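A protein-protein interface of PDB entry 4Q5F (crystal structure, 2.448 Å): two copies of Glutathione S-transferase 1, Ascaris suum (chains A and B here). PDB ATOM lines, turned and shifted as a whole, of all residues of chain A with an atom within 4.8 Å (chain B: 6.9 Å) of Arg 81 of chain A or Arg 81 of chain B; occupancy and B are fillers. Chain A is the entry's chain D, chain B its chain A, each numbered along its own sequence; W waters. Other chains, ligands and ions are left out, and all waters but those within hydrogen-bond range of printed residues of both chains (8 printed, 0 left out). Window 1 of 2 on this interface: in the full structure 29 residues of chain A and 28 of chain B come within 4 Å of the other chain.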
ATOM      1  N   ALA A  77      11.937 -24.655  -6.385  1.00  0.00           N
ATOM      2  CA  ALA A  77      11.421 -23.368  -5.928  1.00  0.00           C
ATOM      3  C   ALA A  77      12.547 -22.487  -5.381  1.00  0.00           C
ATOM      4  O   ALA A  77      12.557 -21.274  -5.594  1.00  0.00           O
ATOM      5  CB  ALA A  77      10.337 -23.564  -4.882  1.00  0.00           C
ATOM      6  N   ALA A  78      13.494 -23.102  -4.682  1.00  0.00           N
ATOM      7  CA  ALA A  78      14.658 -22.380  -4.188  1.00  0.00           C
ATOM      8  C   ALA A  78      15.484 -21.884  -5.370  1.00  0.00           C
ATOM      9  O   ALA A  78      16.069 -20.803  -5.320  1.00  0.00           O
ATOM     10  CB  ALA A  78      15.498 -23.272  -3.288  1.00  0.00           C
ATOM     11  N   ILE A  79      15.524 -22.683  -6.434  1.00  0.00           N
ATOM     12  CA  ILE A  79      16.249 -22.311  -7.645  1.00  0.00           C
ATOM     13  C   ILE A  79      15.563 -21.141  -8.346  1.00  0.00           C
ATOM     14  O   ILE A  79      16.224 -20.192  -8.765  1.00  0.00           O
ATOM     15  CB  ILE A  79      16.382 -23.511  -8.615  1.00  0.00           C
ATOM     16  CG1 ILE A  79      17.265 -24.591  -7.989  1.00  0.00           C
ATOM     17  CG2 ILE A  79      16.971 -23.070  -9.955  1.00  0.00           C
ATOM     18  CD1 ILE A  79      17.247 -25.916  -8.725  1.00  0.00           C
ATOM     19  N   TYR A  80      14.240 -21.214  -8.477  1.00  0.00           N
ATOM     20  CA  TYR A  80      13.472 -20.139  -9.095  1.00  0.00           C
ATOM     21  C   TYR A  80      13.736 -18.819  -8.379  1.00  0.00           C
ATOM     22  O   TYR A  80      14.026 -17.803  -9.009  1.00  0.00           O
ATOM     23  CB  TYR A  80      11.970 -20.424  -9.031  1.00  0.00           C
ATOM     24  CG  TYR A  80      11.514 -21.729  -9.648  1.00  0.00           C
ATOM     25  CD1 TYR A  80      12.256 -22.362 -10.636  1.00  0.00           C
ATOM     26  CD2 TYR A  80      10.321 -22.321  -9.246  1.00  0.00           C
ATOM     27  CE1 TYR A  80      11.827 -23.552 -11.199  1.00  0.00           C
ATOM     28  CE2 TYR A  80       9.888 -23.507  -9.799  1.00  0.00           C
ATOM     29  CZ  TYR A  80      10.642 -24.116 -10.776  1.00  0.00           C
ATOM     30  OH  TYR A  80      10.208 -25.297 -11.327  1.00  0.00           O
ATOM     31  N   ARG A  81      13.625 -18.851  -7.055  1.00  0.00           N
ATOM     32  CA  ARG A  81      13.742 -17.651  -6.239  1.00  0.00           C
ATOM     33  C   ARG A  81      15.152 -17.076  -6.303  1.00  0.00           C
ATOM     34  O   ARG A  81      15.335 -15.859  -6.377  1.00  0.00           O
ATOM     35  CB  ARG A  81      13.373 -17.966  -4.787  1.00  0.00           C
ATOM     36  CG  ARG A  81      13.332 -16.740  -3.881  1.00  0.00           C
ATOM     37  CD  ARG A  81      12.777 -17.065  -2.500  1.00  0.00           C
ATOM     38  NE  ARG A  81      11.492 -17.764  -2.574  1.00  0.00           N
ATOM     39  CZ  ARG A  81      11.324 -19.077  -2.422  1.00  0.00           C
ATOM     40  NH1 ARG A  81      12.356 -19.877  -2.168  1.00  0.00           N
ATOM     41  NH2 ARG A  81      10.110 -19.598  -2.517  1.00  0.00           N
ATOM     42  N   TYR A  82      16.146 -17.956  -6.270  1.00  0.00           N
ATOM     43  CA  TYR A  82      17.535 -17.525  -6.325  1.00  0.00           C
ATOM     44  C   TYR A  82      17.813 -16.808  -7.642  1.00  0.00           C
ATOM     45  O   TYR A  82      18.385 -15.719  -7.658  1.00  0.00           O
ATOM     46  CB  TYR A  82      18.482 -18.715  -6.167  1.00  0.00           C
ATOM     47  CG  TYR A  82      19.936 -18.336  -6.311  1.00  0.00           C
ATOM     48  CD1 TYR A  82      20.628 -17.753  -5.258  1.00  0.00           C
ATOM     49  CD2 TYR A  82      20.615 -18.552  -7.501  1.00  0.00           C
ATOM     50  CE1 TYR A  82      21.959 -17.398  -5.387  1.00  0.00           C
ATOM     51  CE2 TYR A  82      21.945 -18.201  -7.640  1.00  0.00           C
ATOM     52  CZ  TYR A  82      22.611 -17.625  -6.580  1.00  0.00           C
ATOM     53  OH  TYR A  82      23.934 -17.273  -6.710  1.00  0.00           O
ATOM     54  N   LEU A  83      17.402 -17.425  -8.744  1.00  0.00           N
ATOM     55  CA  LEU A  83      17.550 -16.820 -10.060  1.00  0.00           C
ATOM     56  C   LEU A  83      16.754 -15.527 -10.159  1.00  0.00           C
ATOM     57  O   LEU A  83      17.232 -14.530 -10.698  1.00  0.00           O
ATOM     58  CB  LEU A  83      17.084 -17.794 -11.145  1.00  0.00           C
ATOM     59  CG  LEU A  83      18.125 -18.778 -11.680  1.00  0.00           C
ATOM     60  CD1 LEU A  83      19.003 -19.324 -10.575  1.00  0.00           C
ATOM     61  CD2 LEU A  83      17.441 -19.920 -12.417  1.00  0.00           C
ATOM     62  N   GLY A  84      15.532 -15.555  -9.639  1.00  0.00           N
ATOM     63  CA  GLY A  84      14.650 -14.406  -9.699  1.00  0.00           C
ATOM     64  C   GLY A  84      15.250 -13.181  -9.041  1.00  0.00           C
ATOM     65  O   GLY A  84      15.215 -12.086  -9.601  1.00  0.00           O
ATOM     66  N   ARG A  85      15.803 -13.372  -7.848  1.00  0.00           N
ATOM     67  CA  ARG A  85      16.404 -12.278  -7.097  1.00  0.00           C
ATOM     68  C   ARG A  85      17.684 -11.787  -7.761  1.00  0.00           C
ATOM     69  O   ARG A  85      17.952 -10.586  -7.793  1.00  0.00           O
ATOM     70  CB  ARG A  85      16.678 -12.721  -5.661  1.00  0.00           C
ATOM     71  CG  ARG A  85      15.420 -12.802  -4.820  1.00  0.00           C
ATOM     72  CD  ARG A  85      15.575 -13.700  -3.608  1.00  0.00           C
ATOM     73  NE  ARG A  85      16.412 -13.099  -2.573  1.00  0.00           N
ATOM     74  CZ  ARG A  85      16.258 -13.303  -1.266  1.00  0.00           C
ATOM     75  NH1 ARG A  85      15.289 -14.092  -0.812  1.00  0.00           N
ATOM     76  NH2 ARG A  85      17.074 -12.711  -0.403  1.00  0.00           N
ATOM     77  N   ASP A 101       6.345 -14.942  -3.456  1.00  0.00           N
ATOM     78  CA  ASP A 101       6.469 -16.245  -2.815  1.00  0.00           C
ATOM     79  C   ASP A 101       5.094 -16.802  -2.471  1.00  0.00           C
ATOM     80  O   ASP A 101       4.840 -17.999  -2.616  1.00  0.00           O
ATOM     81  CB  ASP A 101       7.299 -16.142  -1.533  1.00  0.00           C
ATOM     82  CG  ASP A 101       8.766 -15.884  -1.801  1.00  0.00           C
ATOM     83  OD1 ASP A 101       9.187 -15.956  -2.975  1.00  0.00           O
ATOM     84  OD2 ASP A 101       9.502 -15.623  -0.827  1.00  0.00           O
ATOM     85  N   TRP A 167       9.393 -14.092 -11.480  1.00  0.00           N
ATOM     86  CA  TRP A 167       9.694 -15.497 -11.738  1.00  0.00           C
ATOM     87  C   TRP A 167       8.481 -16.387 -11.490  1.00  0.00           C
ATOM     88  O   TRP A 167       8.328 -17.425 -12.131  1.00  0.00           O
ATOM     89  CB  TRP A 167      10.880 -15.971 -10.891  1.00  0.00           C
ATOM     90  CG  TRP A 167      10.657 -15.908  -9.406  1.00  0.00           C
ATOM     91  CD1 TRP A 167      11.024 -14.898  -8.564  1.00  0.00           C
ATOM     92  CD2 TRP A 167      10.033 -16.904  -8.584  1.00  0.00           C
ATOM     93  NE1 TRP A 167      10.664 -15.201  -7.274  1.00  0.00           N
ATOM     94  CE2 TRP A 167      10.054 -16.427  -7.260  1.00  0.00           C
ATOM     95  CE3 TRP A 167       9.456 -18.151  -8.844  1.00  0.00           C
ATOM     96  CZ2 TRP A 167       9.520 -17.152  -6.196  1.00  0.00           C
ATOM     97  CZ3 TRP A 167       8.928 -18.868  -7.786  1.00  0.00           C
ATOM     98  CH2 TRP A 167       8.963 -18.368  -6.479  1.00  0.00           C
ATOM     99  N   ILE B  33       9.952 -17.622  15.127  1.00  0.00           N
ATOM    100  CA  ILE B  33      10.826 -16.656  14.468  1.00  0.00           C
ATOM    101  C   ILE B  33      10.748 -15.299  15.171  1.00  0.00           C
ATOM    102  O   ILE B  33      11.762 -14.621  15.332  1.00  0.00           O
ATOM    103  CB  ILE B  33      10.474 -16.516  12.970  1.00  0.00           C
ATOM    104  CG1 ILE B  33      10.755 -17.831  12.240  1.00  0.00           C
ATOM    105  CG2 ILE B  33      11.292 -15.408  12.314  1.00  0.00           C
ATOM    106  CD1 ILE B  33      10.038 -17.967  10.911  1.00  0.00           C
ATOM    107  N   SER B  76       2.332 -19.925   4.840  1.00  0.00           N
ATOM    108  CA  SER B  76       3.272 -20.076   5.953  1.00  0.00           C
ATOM    109  C   SER B  76       4.742 -19.907   5.564  1.00  0.00           C
ATOM    110  O   SER B  76       5.475 -19.161   6.212  1.00  0.00           O
ATOM    111  CB  SER B  76       3.078 -21.442   6.617  1.00  0.00           C
ATOM    112  OG  SER B  76       3.275 -22.496   5.689  1.00  0.00           O
ATOM    113  N   ALA B  77       5.176 -20.605   4.520  1.00  0.00           N
ATOM    114  CA  ALA B  77       6.579 -20.566   4.121  1.00  0.00           C
ATOM    115  C   ALA B  77       6.995 -19.161   3.689  1.00  0.00           C
ATOM    116  O   ALA B  77       8.104 -18.719   3.981  1.00  0.00           O
ATOM    117  CB  ALA B  77       6.847 -21.567   3.006  1.00  0.00           C
ATOM    118  N   ALA B  78       6.102 -18.463   2.995  1.00  0.00           N
ATOM    119  CA  ALA B  78       6.364 -17.090   2.580  1.00  0.00           C
ATOM    120  C   ALA B  78       6.444 -16.192   3.809  1.00  0.00           C
ATOM    121  O   ALA B  78       7.178 -15.204   3.827  1.00  0.00           O
ATOM    122  CB  ALA B  78       5.276 -16.604   1.631  1.00  0.00           C
ATOM    123  N   ILE B  79       5.681 -16.547   4.838  1.00  0.00           N
ATOM    124  CA  ILE B  79       5.699 -15.813   6.097  1.00  0.00           C
ATOM    125  C   ILE B  79       7.008 -16.070   6.845  1.00  0.00           C
ATOM    126  O   ILE B  79       7.605 -15.144   7.394  1.00  0.00           O
ATOM    127  CB  ILE B  79       4.486 -16.182   6.983  1.00  0.00           C
ATOM    128  CG1 ILE B  79       3.211 -15.589   6.380  1.00  0.00           C
ATOM    129  CG2 ILE B  79       4.671 -15.676   8.415  1.00  0.00           C
ATOM    130  CD1 ILE B  79       1.929 -16.089   7.015  1.00  0.00           C
ATOM    131  N   TYR B  80       7.448 -17.326   6.867  1.00  0.00           N
ATOM    132  CA  TYR B  80       8.703 -17.678   7.522  1.00  0.00           C
ATOM    133  C   TYR B  80       9.854 -16.885   6.919  1.00  0.00           C
ATOM    134  O   TYR B  80      10.635 -16.255   7.634  1.00  0.00           O
ATOM    135  CB  TYR B  80       9.015 -19.166   7.359  1.00  0.00           C
ATOM    136  CG  TYR B  80       7.960 -20.128   7.865  1.00  0.00           C
ATOM    137  CD1 TYR B  80       7.006 -19.733   8.793  1.00  0.00           C
ATOM    138  CD2 TYR B  80       7.933 -21.445   7.418  1.00  0.00           C
ATOM    139  CE1 TYR B  80       6.047 -20.622   9.252  1.00  0.00           C
ATOM    140  CE2 TYR B  80       6.984 -22.336   7.871  1.00  0.00           C
ATOM    141  CZ  TYR B  80       6.044 -21.923   8.788  1.00  0.00           C
ATOM    142  OH  TYR B  80       5.100 -22.818   9.234  1.00  0.00           O
ATOM    143  N   ARG B  81       9.947 -16.926   5.593  1.00  0.00           N
ATOM    144  CA  ARG B  81      11.069 -16.333   4.881  1.00  0.00           C
ATOM    145  C   ARG B  81      11.062 -14.814   4.993  1.00  0.00           C
ATOM    146  O   ARG B  81      12.109 -14.195   5.180  1.00  0.00           O
ATOM    147  CB  ARG B  81      11.042 -16.751   3.411  1.00  0.00           C
ATOM    148  CG  ARG B  81      12.266 -16.310   2.627  1.00  0.00           C
ATOM    149  CD  ARG B  81      12.246 -16.834   1.196  1.00  0.00           C
ATOM    150  NE  ARG B  81      12.056 -18.285   1.143  1.00  0.00           N
ATOM    151  CZ  ARG B  81      10.906 -18.899   0.873  1.00  0.00           C
ATOM    152  NH1 ARG B  81       9.803 -18.206   0.611  1.00  0.00           N
ATOM    153  NH2 ARG B  81      10.858 -20.222   0.859  1.00  0.00           N
ATOM    154  N   TYR B  82       9.881 -14.216   4.879  1.00  0.00           N
ATOM    155  CA  TYR B  82       9.756 -12.770   5.005  1.00  0.00           C
ATOM    156  C   TYR B  82      10.254 -12.310   6.374  1.00  0.00           C
ATOM    157  O   TYR B  82      11.057 -11.385   6.469  1.00  0.00           O
ATOM    158  CB  TYR B  82       8.309 -12.319   4.798  1.00  0.00           C
ATOM    159  CG  TYR B  82       8.096 -10.857   5.110  1.00  0.00           C
ATOM    160  CD1 TYR B  82       8.290  -9.883   4.139  1.00  0.00           C
ATOM    161  CD2 TYR B  82       7.711 -10.447   6.380  1.00  0.00           C
ATOM    162  CE1 TYR B  82       8.102  -8.543   4.424  1.00  0.00           C
ATOM    163  CE2 TYR B  82       7.521  -9.110   6.674  1.00  0.00           C
ATOM    164  CZ  TYR B  82       7.718  -8.163   5.692  1.00  0.00           C
ATOM    165  OH  TYR B  82       7.529  -6.831   5.978  1.00  0.00           O
ATOM    166  N   LEU B  83       9.780 -12.964   7.429  1.00  0.00           N
ATOM    167  CA  LEU B  83      10.177 -12.608   8.787  1.00  0.00           C
ATOM    168  C   LEU B  83      11.666 -12.861   9.008  1.00  0.00           C
ATOM    169  O   LEU B  83      12.367 -12.035   9.595  1.00  0.00           O
ATOM    170  CB  LEU B  83       9.358 -13.399   9.807  1.00  0.00           C
ATOM    171  CG  LEU B  83       7.857 -13.107   9.827  1.00  0.00           C
ATOM    172  CD1 LEU B  83       7.129 -14.101  10.722  1.00  0.00           C
ATOM    173  CD2 LEU B  83       7.587 -11.683  10.287  1.00  0.00           C
ATOM    174  N   GLY B  84      12.140 -14.007   8.536  1.00  0.00           N
ATOM    175  CA  GLY B  84      13.536 -14.377   8.688  1.00  0.00           C
ATOM    176  C   GLY B  84      14.475 -13.357   8.073  1.00  0.00           C
ATOM    177  O   GLY B  84      15.504 -13.018   8.657  1.00  0.00           O
ATOM    178  N   ARG B  85      14.121 -12.863   6.893  1.00  0.00           N
ATOM    179  CA  ARG B  85      14.930 -11.858   6.215  1.00  0.00           C
ATOM    180  C   ARG B  85      14.895 -10.519   6.948  1.00  0.00           C
ATOM    181  O   ARG B  85      15.882  -9.785   6.954  1.00  0.00           O
ATOM    182  CB  ARG B  85      14.461 -11.676   4.770  1.00  0.00           C
ATOM    183  CG  ARG B  85      15.141 -12.612   3.779  1.00  0.00           C
ATOM    184  CD  ARG B  85      14.551 -12.500   2.381  1.00  0.00           C
ATOM    185  NE  ARG B  85      14.331 -11.117   1.970  1.00  0.00           N
ATOM    186  CZ  ARG B  85      13.897 -10.753   0.768  1.00  0.00           C
ATOM    187  NH1 ARG B  85      13.640 -11.670  -0.156  1.00  0.00           N
ATOM    188  NH2 ARG B  85      13.722  -9.470   0.485  1.00  0.00           N
ATOM    189  N   GLN B  86      13.758 -10.203   7.562  1.00  0.00           N
ATOM    190  CA  GLN B  86      13.619  -8.954   8.303  1.00  0.00           C
ATOM    191  C   GLN B  86      14.494  -8.945   9.552  1.00  0.00           C
ATOM    192  O   GLN B  86      14.993  -7.895   9.956  1.00  0.00           O
ATOM    193  CB  GLN B  86      12.158  -8.718   8.705  1.00  0.00           C
ATOM    194  CG  GLN B  86      11.237  -8.302   7.566  1.00  0.00           C
ATOM    195  CD  GLN B  86      11.718  -7.060   6.842  1.00  0.00           C
ATOM    196  OE1 GLN B  86      11.677  -5.956   7.382  1.00  0.00           O
ATOM    197  NE2 GLN B  86      12.182  -7.240   5.612  1.00  0.00           N
ATOM    198  N   LEU B  89      17.598 -13.622   9.992  1.00  0.00           N
ATOM    199  CA  LEU B  89      17.537 -15.050  10.291  1.00  0.00           C
ATOM    200  C   LEU B  89      17.329 -15.869   9.019  1.00  0.00           C
ATOM    201  O   LEU B  89      16.845 -17.002   9.073  1.00  0.00           O
ATOM    202  CB  LEU B  89      16.392 -15.332  11.268  1.00  0.00           C
ATOM    203  CG  LEU B  89      16.478 -14.659  12.639  1.00  0.00           C
ATOM    204  CD1 LEU B  89      15.178 -14.852  13.406  1.00  0.00           C
ATOM    205  CD2 LEU B  89      17.654 -15.205  13.433  1.00  0.00           C
ATOM    206  N   ALA B  90      17.701 -15.295   7.877  1.00  0.00           N
ATOM    207  CA  ALA B  90      17.429 -15.913   6.582  1.00  0.00           C
ATOM    208  C   ALA B  90      18.683 -16.482   5.920  1.00  0.00           C
ATOM    209  O   ALA B  90      18.588 -17.256   4.970  1.00  0.00           O
ATOM    210  CB  ALA B  90      16.763 -14.906   5.657  1.00  0.00           C
ATOM    211  N   GLU B  97      21.006 -17.985   1.760  1.00  0.00           N
ATOM    212  CA  GLU B  97      19.560 -17.837   1.835  1.00  0.00           C
ATOM    213  C   GLU B  97      18.864 -18.892   0.985  1.00  0.00           C
ATOM    214  O   GLU B  97      17.881 -19.501   1.413  1.00  0.00           O
ATOM    215  CB  GLU B  97      19.135 -16.441   1.379  1.00  0.00           C
ATOM    216  CG  GLU B  97      19.471 -15.333   2.363  1.00  0.00           C
ATOM    217  CD  GLU B  97      19.049 -13.966   1.858  1.00  0.00           C
ATOM    218  OE1 GLU B  97      17.845 -13.643   1.949  1.00  0.00           O
ATOM    219  OE2 GLU B  97      19.919 -13.218   1.363  1.00  0.00           O
ATOM    220  N   ALA B  98      19.377 -19.102  -0.224  1.00  0.00           N
ATOM    221  CA  ALA B  98      18.823 -20.103  -1.122  1.00  0.00           C
ATOM    222  C   ALA B  98      18.997 -21.501  -0.535  1.00  0.00           C
ATOM    223  O   ALA B  98      18.147 -22.370  -0.722  1.00  0.00           O
ATOM    224  CB  ALA B  98      19.483 -20.013  -2.483  1.00  0.00           C
ATOM    225  N   VAL B 100      19.052 -22.169   2.703  1.00  0.00           N
ATOM    226  CA  VAL B 100      18.043 -22.265   3.753  1.00  0.00           C
ATOM    227  C   VAL B 100      16.712 -22.686   3.130  1.00  0.00           C
ATOM    228  O   VAL B 100      16.007 -23.542   3.671  1.00  0.00           O
ATOM    229  CB  VAL B 100      17.894 -20.920   4.518  1.00  0.00           C
ATOM    230  CG1 VAL B 100      16.623 -20.884   5.379  1.00  0.00           C
ATOM    231  CG2 VAL B 100      19.110 -20.669   5.390  1.00  0.00           C
ATOM    232  N   ASP B 101      16.372 -22.084   1.994  1.00  0.00           N
ATOM    233  CA  ASP B 101      15.147 -22.432   1.287  1.00  0.00           C
ATOM    234  C   ASP B 101      15.168 -23.888   0.835  1.00  0.00           C
ATOM    235  O   ASP B 101      14.148 -24.577   0.887  1.00  0.00           O
ATOM    236  CB  ASP B 101      14.952 -21.537   0.061  1.00  0.00           C
ATOM    237  CG  ASP B 101      14.658 -20.098   0.426  1.00  0.00           C
ATOM    238  OD1 ASP B 101      14.376 -19.823   1.610  1.00  0.00           O
ATOM    239  OD2 ASP B 101      14.696 -19.240  -0.481  1.00  0.00           O
ATOM    240  N   SER B 102      16.334 -24.348   0.393  1.00  0.00           N
ATOM    241  CA  SER B 102      16.467 -25.679  -0.184  1.00  0.00           C
ATOM    242  C   SER B 102      16.224 -26.771   0.848  1.00  0.00           C
ATOM    243  O   SER B 102      15.483 -27.718   0.590  1.00  0.00           O
ATOM    244  CB  SER B 102      17.854 -25.856  -0.807  1.00  0.00           C
ATOM    245  OG  SER B 102      17.955 -27.100  -1.476  1.00  0.00           O
ATOM    246  N   PHE B 104      14.662 -26.498   3.622  1.00  0.00           N
ATOM    247  CA  PHE B 104      13.292 -26.394   4.102  1.00  0.00           C
ATOM    248  C   PHE B 104      12.313 -26.991   3.096  1.00  0.00           C
ATOM    249  O   PHE B 104      11.311 -27.595   3.475  1.00  0.00           O
ATOM    250  CB  PHE B 104      12.913 -24.943   4.391  1.00  0.00           C
ATOM    251  CG  PHE B 104      11.523 -24.791   4.931  1.00  0.00           C
ATOM    252  CD1 PHE B 104      11.230 -25.181   6.223  1.00  0.00           C
ATOM    253  CD2 PHE B 104      10.507 -24.277   4.145  1.00  0.00           C
ATOM    254  CE1 PHE B 104       9.951 -25.055   6.727  1.00  0.00           C
ATOM    255  CE2 PHE B 104       9.225 -24.147   4.644  1.00  0.00           C
ATOM    256  CZ  PHE B 104       8.948 -24.536   5.937  1.00  0.00           C
ATOM    257  N   ASP B 105      12.600 -26.809   1.811  1.00  0.00           N
ATOM    258  CA  ASP B 105      11.773 -27.395   0.765  1.00  0.00           C
ATOM    259  C   ASP B 105      11.876 -28.915   0.794  1.00  0.00           C
ATOM    260  O   ASP B 105      10.904 -29.613   0.508  1.00  0.00           O
ATOM    261  CB  ASP B 105      12.182 -26.867  -0.611  1.00  0.00           C
ATOM    262  CG  ASP B 105      11.388 -25.643  -1.031  1.00  0.00           C
ATOM    263  OD1 ASP B 105      10.643 -25.079  -0.202  1.00  0.00           O
ATOM    264  OD2 ASP B 105      11.518 -25.239  -2.204  1.00  0.00           O
ATOM    265  N   TRP B 167      15.600 -19.350  10.190  1.00  0.00           N
ATOM    266  CA  TRP B 167      14.177 -19.635  10.344  1.00  0.00           C
ATOM    267  C   TRP B 167      13.846 -21.088  10.015  1.00  0.00           C
ATOM    268  O   TRP B 167      12.921 -21.661  10.587  1.00  0.00           O
ATOM    269  CB  TRP B 167      13.326 -18.689   9.488  1.00  0.00           C
ATOM    270  CG  TRP B 167      13.587 -18.760   8.005  1.00  0.00           C
ATOM    271  CD1 TRP B 167      14.430 -17.965   7.284  1.00  0.00           C
ATOM    272  CD2 TRP B 167      12.985 -19.662   7.066  1.00  0.00           C
ATOM    273  NE1 TRP B 167      14.394 -18.318   5.957  1.00  0.00           N
ATOM    274  CE2 TRP B 167      13.516 -19.357   5.797  1.00  0.00           C
ATOM    275  CE3 TRP B 167      12.055 -20.699   7.173  1.00  0.00           C
ATOM    276  CZ2 TRP B 167      13.148 -20.051   4.648  1.00  0.00           C
ATOM    277  CZ3 TRP B 167      11.691 -21.385   6.031  1.00  0.00           C
ATOM    278  CH2 TRP B 167      12.237 -21.059   4.785  1.00  0.00           C
HETATM  279  O   HOH W   1      16.217 -19.299  -3.072  1.00  0.00           O
HETATM  280  O   HOH W   2      11.355 -26.591  -4.295  1.00  0.00           O
HETATM  281  O   HOH W   3       8.767 -14.428   1.549  1.00  0.00           O
HETATM  282  O   HOH W   4      11.709 -22.424  -1.630  1.00  0.00           O
HETATM  283  O   HOH W   5      11.462 -13.812  -1.100  1.00  0.00           O
HETATM  284  O   HOH W   6      15.528 -16.909  -0.026  1.00  0.00           O
HETATM  285  O   HOH W   7      15.824 -15.401   2.005  1.00  0.00           O
HETATM  286  O   HOH W   8       8.851 -21.759  -0.332  1.00  0.00           O
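The side-chain carboxylate of Glu 97 of chain B is in salt-bridge range of the guanidinium group of Arg 85 of chain A (2.6 Å). NH1 of Arg 81 of chain A lies within salt-bridge range of OD2 of Asp 101 of chain B, at 3.0 Å. NH1 of Arg 81 of chain B is in salt-bridge range of OD2 of Asp 101 of chain A, at 3.0 Å. The guanidinium group of Arg 81 of chain B sits close to the guanidinium group of Arg 81 of chain A (3.4 Å). NH1 of Arg 85 of chain A lies close to NH1 of Arg 85 of chain B (3.0 Å).
OD1 of Asp 101 of chain A is in salt-bridge range of NE of Arg 81 of chain A (3.0 Å). The guanidinium group (NE) of Arg 81 of chain B is in salt-bridge range of the side-chain carboxylate (OD1) of Asp 101 of chain B (2.8 Å).
CB of Ala 77 of chain A touches OD2 of Asp 105 of chain B, 3.4 Å away. Ala 78 of chain A touches Ala 98 of chain B. Asp 101 of chain B touches Ala 78 of chain A (CB to CB, 3.8 Å). CB of Ala 78 of chain A touches N of Ser 102 of chain B, 3.9 Å away. Ala 78 of chain A touches Asp 105 of chain B (N to OD2, 3.8 Å). CD1 of Tyr 82 of chain A touches CB of Ala 98 of chain B, at 3.8 Å. Ala 78 of chain B touches Asp 101 of chain A.
Arg 81 of chain A touches just these residues of chain B: Arg 81 (3.3 Å) and Asp 101 (3.0 Å). Printed residues of chain B within 4 Å of Arg 85 of chain A: Arg 85 (3.0 Å) and Glu 97 (2.6 Å). Of the printed residues of chain B, Asp 101 of chain A touches Ala 78 (3.8 Å) and Arg 81 (3.0 Å). Arg 81 of chain B touches two residues of chain A. Of the printed residues of chain A, Asp 101 of chain B touches Ala 78 (3.8 Å) and Arg 81 (3.0 Å). Of the printed residues of chain A, Ser 102 of chain B touches Ala 78. Printed residues of chain A within 4 Å of Asp 105 of chain B: Ala 77 and Ala 78. The nearest residue of chain B that does not touch Arg 81 of chain A is Asp 105 of chain B (5.4 Å). The nearest residue of chain A that does not touch Arg 81 of chain B is Arg 85 of chain A (4.6 Å).
Of the 11 printed residues of chain A, 6 touch a printed residue of chain B. Printed residues of chain A that touch a printed residue of chain B: Ala 77, Ala 78, Arg 81, Tyr 82, Arg 85 and Asp 101. Hydrophobic or aromatic side chains of chain A within 4 Å of the printed part of chain B: Ala 77, Ala 78 and Tyr 82. Among the printed residues, Asp or Glu carboxylates within 4 Å of a Lys or Arg side-chain nitrogen of the other chain: Arg 81 of chain A with Asp 101 of chain B (3.0 Å), Arg 85 of chain A with Glu 97 of chain B (2.6 Å) and Asp 101 of chain A with Arg 81 of chain B (3.0 Å).
Ala 78 of chain A touches Asp 101 of chain B, and with the chains exchanged Asp 101 of chain A touches Ala 78 of chain B. Arg 81 of chain A touches its own counterpart, Arg 81 of chain B. Arg 81 of chain A touches Asp 101 of chain B, and with the chains exchanged Asp 101 of chain A touches Arg 81 of chain B. Arg 85 of chain A touches its own counterpart, Arg 85 of chain B. 11 positions are printed for both chains. Of the 12 pairs that touch across the chains among the printed residues, 6 have their exchanged pair printed and touching as well.
Water W2 lies within hydrogen-bond range of the side-chain carboxylate (OD2) of Asp 105 of chain B (2.5 Å) and the backbone NH (N) of Ala 77 of chain A (2.9 Å). Water W6 bridges OD2 of Asp 101 of chain B (2.5 Å) and NH1 of Arg 85 of chain A (2.9 Å). Water W7 bridges OE1 of Glu 97 of chain B (2.7 Å) and NH1 of Arg 85 of chain A (3.2 Å). Water W4 lies within hydrogen-bond range of the guanidinium group of Arg 81 of chain A, the side-chain carboxylate of Asp 105 of chain B and the guanidinium group of Arg 81 of chain B. Water W5 bridges OD2 of Asp 101 of chain A (2.7 Å) and NH1 of Arg 85 of chain B (3.2 Å). Water W3 bridges OD2 of Asp 101 of chain A (2.8 Å) and O of Ala 78 of chain B (2.9 Å).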
